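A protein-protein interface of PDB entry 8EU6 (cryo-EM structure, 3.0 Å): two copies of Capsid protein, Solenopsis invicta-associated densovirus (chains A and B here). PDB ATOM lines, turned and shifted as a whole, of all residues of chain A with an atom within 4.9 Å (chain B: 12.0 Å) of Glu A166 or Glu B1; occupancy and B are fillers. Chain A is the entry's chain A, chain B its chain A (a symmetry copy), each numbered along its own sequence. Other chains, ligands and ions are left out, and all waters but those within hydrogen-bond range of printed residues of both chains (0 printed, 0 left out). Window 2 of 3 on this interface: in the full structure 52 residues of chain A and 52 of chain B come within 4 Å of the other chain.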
ATOM      1  N   ASN A 121       8.199 -18.882   7.284  1.00  0.00           N
ATOM      2  CA  ASN A 121       7.336 -20.003   7.601  1.00  0.00           C
ATOM      3  C   ASN A 121       7.751 -20.602   8.935  1.00  0.00           C
ATOM      4  O   ASN A 121       8.831 -20.326   9.459  1.00  0.00           O
ATOM      5  CB  ASN A 121       7.381 -21.041   6.487  1.00  0.00           C
ATOM      6  CG  ASN A 121       8.777 -21.487   6.172  1.00  0.00           C
ATOM      7  OD1 ASN A 121       9.658 -21.481   7.029  1.00  0.00           O
ATOM      8  ND2 ASN A 121       8.991 -21.877   4.929  1.00  0.00           N
ATOM      9  N   LEU A 122       6.863 -21.425   9.476  1.00  0.00           N
ATOM     10  CA  LEU A 122       7.095 -22.073  10.752  1.00  0.00           C
ATOM     11  C   LEU A 122       8.051 -23.242  10.589  1.00  0.00           C
ATOM     12  O   LEU A 122       8.110 -23.881   9.537  1.00  0.00           O
ATOM     13  CB  LEU A 122       5.778 -22.564  11.333  1.00  0.00           C
ATOM     14  CG  LEU A 122       5.867 -23.325  12.643  1.00  0.00           C
ATOM     15  CD1 LEU A 122       6.403 -22.428  13.708  1.00  0.00           C
ATOM     16  CD2 LEU A 122       4.521 -23.842  13.033  1.00  0.00           C
ATOM     17  N   PHE A 123       8.801 -23.523  11.649  1.00  0.00           N
ATOM     18  CA  PHE A 123       9.781 -24.596  11.662  1.00  0.00           C
ATOM     19  C   PHE A 123       9.383 -25.654  12.678  1.00  0.00           C
ATOM     20  O   PHE A 123       8.980 -25.325  13.797  1.00  0.00           O
ATOM     21  CB  PHE A 123      11.168 -24.063  12.001  1.00  0.00           C
ATOM     22  CG  PHE A 123      11.732 -23.149  10.970  1.00  0.00           C
ATOM     23  CD1 PHE A 123      12.347 -23.645   9.845  1.00  0.00           C
ATOM     24  CD2 PHE A 123      11.666 -21.792  11.140  1.00  0.00           C
ATOM     25  CE1 PHE A 123      12.869 -22.801   8.903  1.00  0.00           C
ATOM     26  CE2 PHE A 123      12.187 -20.945  10.206  1.00  0.00           C
ATOM     27  CZ  PHE A 123      12.791 -21.448   9.084  1.00  0.00           C
ATOM     28  N   ILE A 124       9.509 -26.916  12.293  1.00  0.00           N
ATOM     29  CA  ILE A 124       9.265 -28.034  13.189  1.00  0.00           C
ATOM     30  C   ILE A 124      10.620 -28.570  13.608  1.00  0.00           C
ATOM     31  O   ILE A 124      11.291 -29.247  12.824  1.00  0.00           O
ATOM     32  CB  ILE A 124       8.446 -29.137  12.512  1.00  0.00           C
ATOM     33  CG1 ILE A 124       7.203 -28.561  11.852  1.00  0.00           C
ATOM     34  CG2 ILE A 124       8.059 -30.185  13.513  1.00  0.00           C
ATOM     35  CD1 ILE A 124       6.328 -27.818  12.763  1.00  0.00           C
ATOM     36  N   LYS A 164      14.951 -30.056  11.078  1.00  0.00           N
ATOM     37  CA  LYS A 164      13.744 -29.255  11.147  1.00  0.00           C
ATOM     38  C   LYS A 164      13.131 -29.076   9.772  1.00  0.00           C
ATOM     39  O   LYS A 164      13.822 -28.782   8.794  1.00  0.00           O
ATOM     40  CB  LYS A 164      14.028 -27.903  11.787  1.00  0.00           C
ATOM     41  CG  LYS A 164      15.095 -27.112  11.107  1.00  0.00           C
ATOM     42  CD  LYS A 164      15.363 -25.858  11.878  1.00  0.00           C
ATOM     43  CE  LYS A 164      16.495 -25.079  11.286  1.00  0.00           C
ATOM     44  NZ  LYS A 164      17.768 -25.804  11.394  1.00  0.00           N
ATOM     45  N   GLU A 165      11.814 -29.246   9.725  1.00  0.00           N
ATOM     46  CA  GLU A 165      11.027 -29.091   8.514  1.00  0.00           C
ATOM     47  C   GLU A 165      10.268 -27.784   8.635  1.00  0.00           C
ATOM     48  O   GLU A 165       9.694 -27.494   9.689  1.00  0.00           O
ATOM     49  CB  GLU A 165      10.062 -30.259   8.326  1.00  0.00           C
ATOM     50  CG  GLU A 165      10.737 -31.603   8.130  1.00  0.00           C
ATOM     51  CD  GLU A 165       9.746 -32.724   7.919  1.00  0.00           C
ATOM     52  OE1 GLU A 165       8.537 -32.492   8.123  1.00  0.00           O
ATOM     53  OE2 GLU A 165      10.170 -33.834   7.538  1.00  0.00           O
ATOM     54  N   GLU A 166      10.271 -27.000   7.568  1.00  0.00           N
ATOM     55  CA  GLU A 166       9.629 -25.697   7.603  1.00  0.00           C
ATOM     56  C   GLU A 166       8.227 -25.802   7.028  1.00  0.00           C
ATOM     57  O   GLU A 166       8.025 -26.372   5.952  1.00  0.00           O
ATOM     58  CB  GLU A 166      10.454 -24.670   6.834  1.00  0.00           C
ATOM     59  CG  GLU A 166      10.530 -24.914   5.351  1.00  0.00           C
ATOM     60  CD  GLU A 166      11.486 -23.955   4.643  1.00  0.00           C
ATOM     61  OE1 GLU A 166      11.809 -22.894   5.217  1.00  0.00           O
ATOM     62  OE2 GLU A 166      11.915 -24.261   3.513  1.00  0.00           O
ATOM     63  N   VAL A 167       7.260 -25.240   7.743  1.00  0.00           N
ATOM     64  CA  VAL A 167       5.848 -25.389   7.432  1.00  0.00           C
ATOM     65  C   VAL A 167       5.331 -24.055   6.915  1.00  0.00           C
ATOM     66  O   VAL A 167       5.174 -23.105   7.698  1.00  0.00           O
ATOM     67  CB  VAL A 167       5.060 -25.845   8.662  1.00  0.00           C
ATOM     68  CG1 VAL A 167       3.606 -25.956   8.335  1.00  0.00           C
ATOM     69  CG2 VAL A 167       5.595 -27.148   9.146  1.00  0.00           C
ATOM     70  N   PRO A 168       5.042 -23.929   5.629  1.00  0.00           N
ATOM     71  CA  PRO A 168       4.376 -22.736   5.124  1.00  0.00           C
ATOM     72  C   PRO A 168       2.918 -22.706   5.541  1.00  0.00           C
ATOM     73  O   PRO A 168       2.354 -23.688   6.022  1.00  0.00           O
ATOM     74  CB  PRO A 168       4.515 -22.871   3.613  1.00  0.00           C
ATOM     75  CG  PRO A 168       5.682 -23.736   3.428  1.00  0.00           C
ATOM     76  CD  PRO A 168       5.598 -24.727   4.532  1.00  0.00           C
ATOM     77  N   GLU A 171       0.309 -25.081   3.809  1.00  0.00           N
ATOM     78  CA  GLU A 171       0.726 -26.465   3.932  1.00  0.00           C
ATOM     79  C   GLU A 171       0.625 -26.898   5.388  1.00  0.00           C
ATOM     80  O   GLU A 171       0.979 -26.147   6.299  1.00  0.00           O
ATOM     81  CB  GLU A 171       2.155 -26.651   3.420  1.00  0.00           C
ATOM     82  CG  GLU A 171       2.305 -26.400   1.933  1.00  0.00           C
ATOM     83  CD  GLU A 171       3.732 -26.566   1.451  1.00  0.00           C
ATOM     84  OE1 GLU A 171       4.637 -26.698   2.300  1.00  0.00           O
ATOM     85  OE2 GLU A 171       3.948 -26.569   0.221  1.00  0.00           O
ATOM     86  N   GLU B   1       6.840 -24.477  -1.136  1.00  0.00           N
ATOM     87  CA  GLU B   1       8.145 -23.923  -0.792  1.00  0.00           C
ATOM     88  C   GLU B   1       8.669 -24.496   0.522  1.00  0.00           C
ATOM     89  O   GLU B   1       9.839 -24.328   0.860  1.00  0.00           O
ATOM     90  CB  GLU B   1       8.070 -22.396  -0.723  1.00  0.00           C
ATOM     91  CG  GLU B   1       7.180 -21.854   0.381  1.00  0.00           C
ATOM     92  CD  GLU B   1       5.708 -21.977   0.046  1.00  0.00           C
ATOM     93  OE1 GLU B   1       5.387 -22.581  -0.999  1.00  0.00           O
ATOM     94  OE2 GLU B   1       4.873 -21.472   0.822  1.00  0.00           O
ATOM     95  N   GLY B   2       7.791 -25.167   1.265  1.00  0.00           N
ATOM     96  CA  GLY B   2       8.212 -25.906   2.432  1.00  0.00           C
ATOM     97  C   GLY B   2       8.681 -27.302   2.079  1.00  0.00           C
ATOM     98  O   GLY B   2       8.239 -27.892   1.095  1.00  0.00           O
ATOM     99  N   TYR B   3       9.589 -27.835   2.896  1.00  0.00           N
ATOM    100  CA  TYR B   3      10.219 -29.118   2.610  1.00  0.00           C
ATOM    101  C   TYR B   3       9.906 -30.119   3.710  1.00  0.00           C
ATOM    102  O   TYR B   3      10.079 -29.824   4.897  1.00  0.00           O
ATOM    103  CB  TYR B   3      11.732 -28.968   2.438  1.00  0.00           C
ATOM    104  CG  TYR B   3      12.469 -28.367   3.616  1.00  0.00           C
ATOM    105  CD1 TYR B   3      12.865 -29.153   4.684  1.00  0.00           C
ATOM    106  CD2 TYR B   3      12.813 -27.023   3.634  1.00  0.00           C
ATOM    107  CE1 TYR B   3      13.550 -28.616   5.753  1.00  0.00           C
ATOM    108  CE2 TYR B   3      13.500 -26.477   4.695  1.00  0.00           C
ATOM    109  CZ  TYR B   3      13.871 -27.278   5.752  1.00  0.00           C
ATOM    110  OH  TYR B   3      14.558 -26.737   6.815  1.00  0.00           O
ATOM    111  N   GLY B   4       9.420 -31.290   3.306  1.00  0.00           N
ATOM    112  CA  GLY B   4       9.276 -32.441   4.175  1.00  0.00           C
ATOM    113  C   GLY B   4       8.501 -33.536   3.473  1.00  0.00           C
ATOM    114  O   GLY B   4       7.793 -33.263   2.500  1.00  0.00           O
ATOM    115  N   LYS B   5       8.620 -34.780   3.942  1.00  0.00           N
ATOM    116  CA  LYS B   5       7.778 -35.845   3.415  1.00  0.00           C
ATOM    117  C   LYS B   5       6.418 -35.878   4.089  1.00  0.00           C
ATOM    118  O   LYS B   5       5.465 -36.420   3.520  1.00  0.00           O
ATOM    119  CB  LYS B   5       8.465 -37.204   3.574  1.00  0.00           C
ATOM    120  CG  LYS B   5       8.738 -37.618   5.012  1.00  0.00           C
ATOM    121  CD  LYS B   5       9.416 -38.977   5.061  1.00  0.00           C
ATOM    122  CE  LYS B   5       9.698 -39.416   6.483  1.00  0.00           C
ATOM    123  NZ  LYS B   5      10.674 -38.521   7.155  1.00  0.00           N
ATOM    124  N   HIS B   6       6.315 -35.311   5.290  1.00  0.00           N
ATOM    125  CA  HIS B   6       5.045 -35.245   5.993  1.00  0.00           C
ATOM    126  C   HIS B   6       4.192 -34.080   5.516  1.00  0.00           C
ATOM    127  O   HIS B   6       2.963 -34.138   5.608  1.00  0.00           O
ATOM    128  CB  HIS B   6       5.297 -35.131   7.495  1.00  0.00           C
ATOM    129  CG  HIS B   6       5.945 -36.342   8.092  1.00  0.00           C
ATOM    130  ND1 HIS B   6       7.309 -36.537   8.084  1.00  0.00           N
ATOM    131  CD2 HIS B   6       5.415 -37.426   8.705  1.00  0.00           C
ATOM    132  CE1 HIS B   6       7.592 -37.684   8.674  1.00  0.00           C
ATOM    133  NE2 HIS B   6       6.459 -38.246   9.056  1.00  0.00           N
ATOM    134  N   ILE B   7       4.823 -33.023   5.011  1.00  0.00           N
ATOM    135  CA  ILE B   7       4.097 -31.812   4.660  1.00  0.00           C
ATOM    136  C   ILE B   7       3.220 -32.054   3.444  1.00  0.00           C
ATOM    137  O   ILE B   7       3.559 -32.837   2.547  1.00  0.00           O
ATOM    138  CB  ILE B   7       5.076 -30.660   4.399  1.00  0.00           C
ATOM    139  CG1 ILE B   7       5.819 -30.311   5.676  1.00  0.00           C
ATOM    140  CG2 ILE B   7       4.329 -29.459   3.912  1.00  0.00           C
ATOM    141  CD1 ILE B   7       6.969 -29.397   5.461  1.00  0.00           C
ATOM    142  N   THR B   8       2.082 -31.367   3.410  1.00  0.00           N
ATOM    143  CA  THR B   8       1.213 -31.369   2.249  1.00  0.00           C
ATOM    144  C   THR B   8       0.346 -30.121   2.306  1.00  0.00           C
ATOM    145  O   THR B   8       0.165 -29.517   3.364  1.00  0.00           O
ATOM    146  CB  THR B   8       0.346 -32.630   2.193  1.00  0.00           C
ATOM    147  OG1 THR B   8      -0.376 -32.671   0.955  1.00  0.00           O
ATOM    148  CG2 THR B   8      -0.627 -32.653   3.348  1.00  0.00           C
ATOM    149  N   SER B   9      -0.190 -29.743   1.151  1.00  0.00           N
ATOM    150  CA  SER B   9      -1.035 -28.564   1.084  1.00  0.00           C
ATOM    151  C   SER B   9      -2.251 -28.744   1.979  1.00  0.00           C
ATOM    152  O   SER B   9      -2.720 -29.860   2.207  1.00  0.00           O
ATOM    153  CB  SER B   9      -1.472 -28.301  -0.354  1.00  0.00           C
ATOM    154  OG  SER B   9      -2.262 -29.369  -0.848  1.00  0.00           O
ATOM    155  N   MET B  10      -2.757 -27.632   2.497  1.00  0.00           N
ATOM    156  CA  MET B  10      -3.890 -27.687   3.403  1.00  0.00           C
ATOM    157  C   MET B  10      -5.167 -27.988   2.639  1.00  0.00           C
ATOM    158  O   MET B  10      -5.451 -27.373   1.607  1.00  0.00           O
ATOM    159  CB  MET B  10      -4.046 -26.386   4.178  1.00  0.00           C
ATOM    160  CG  MET B  10      -3.068 -26.227   5.309  1.00  0.00           C
ATOM    161  SD  MET B  10      -3.195 -24.612   6.070  1.00  0.00           S
ATOM    162  CE  MET B  10      -4.813 -24.774   6.792  1.00  0.00           C
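Printed residues of chain A that touch a printed residue of chain B: Lys A164, Glu A165, Glu A166, Pro A168 and Glu A171. Hydrophobic or aromatic side chains of chain B within 4 Å of the printed part of chain A: Tyr B3, His B6, Ile B7 and Met B10. Among the printed residues, 16 pairs touch across the chains.
Among the printed residues, pairs that only touch across the chains: Glu A166 with Tyr B3 (2.9 Å), Pro A168 with Glu B1 (3.1 Å), Glu A171 with Thr B8 (3.2 Å), Glu A171 with Ile B7 (3.2 Å), Glu A166 with Ile B7 (3.2 Å), Pro A168 with Gly B2 (3.3 Å), Glu A165 with Tyr B3 (3.5 Å), Glu A166 with Gly B2 (3.6 Å), Glu A171 with Gly B2 (3.7 Å), Glu A165 with Gly B4 (3.7 Å), Glu A171 with Met B10 (3.8 Å), Glu A171 with Glu B1 (3.8 Å), Glu A171 with Ser B9 (3.95 Å) and Glu A165 with His B6 (3.97 Å).
No position is printed for both chains. Of the 16 pairs that touch across the chains among the printed residues, none has its exchanged pair printed and touching as well.
The side-chain hydroxyl (OH) of Tyr B3 lies within hydrogen-bond range of the backbone carbonyl oxygen (O) of Lys A164, at 2.9 Å. O of Glu B1 lies close to OE2 of Glu A166 (3.4 Å).
Glu A166 touches just these residues of chain B: Glu B1 (3.4 Å), Gly B2 (3.6 Å), Tyr B3 (2.9 Å) and Ile B7 (3.2 Å). Of the printed residues of chain A, Glu B1 touches Glu A166, Pro A168 and Glu A171. No residue of chain B comes within 4 Å of Asn A121. No residue of chain B comes within 4 Å of Leu A122. No residue of chain B comes within 4 Å of Phe A123. No residue of chain B comes within 4 Å of Ile A124. No residue of chain B comes within 4 Å of Val A167. Pro A168 touches just these residues of chain B: Glu B1 and Gly B2. Of the printed residues of chain A, Gly B2 touches Glu A166 (3.6 Å), Pro A168 (3.3 Å) and Glu A171 (3.7 Å). Printed residues of chain A within 4 Å of Gly B4: Glu A165 (3.7 Å). Of the printed residues of chain A, Ile B7 touches Glu A166 (3.2 Å) and Glu A171 (3.2 Å). Printed residues of chain A within 4 Å of Thr B8: Glu A171. Lys B5 touches none of the printed residues of chain A. The nearest residue of chain B that does not touch Glu A166 is Gly B4 (5.8 Å).
The side-chain carboxylate (OE1) of Glu A166 sits at hydrogen-bond distance from the side-chain amide nitrogen (ND2) of Asn A121. The backbone NH (N) of Ile A124 is in hydrogen-bond range of the backbone carbonyl oxygen (O) of Glu A165.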
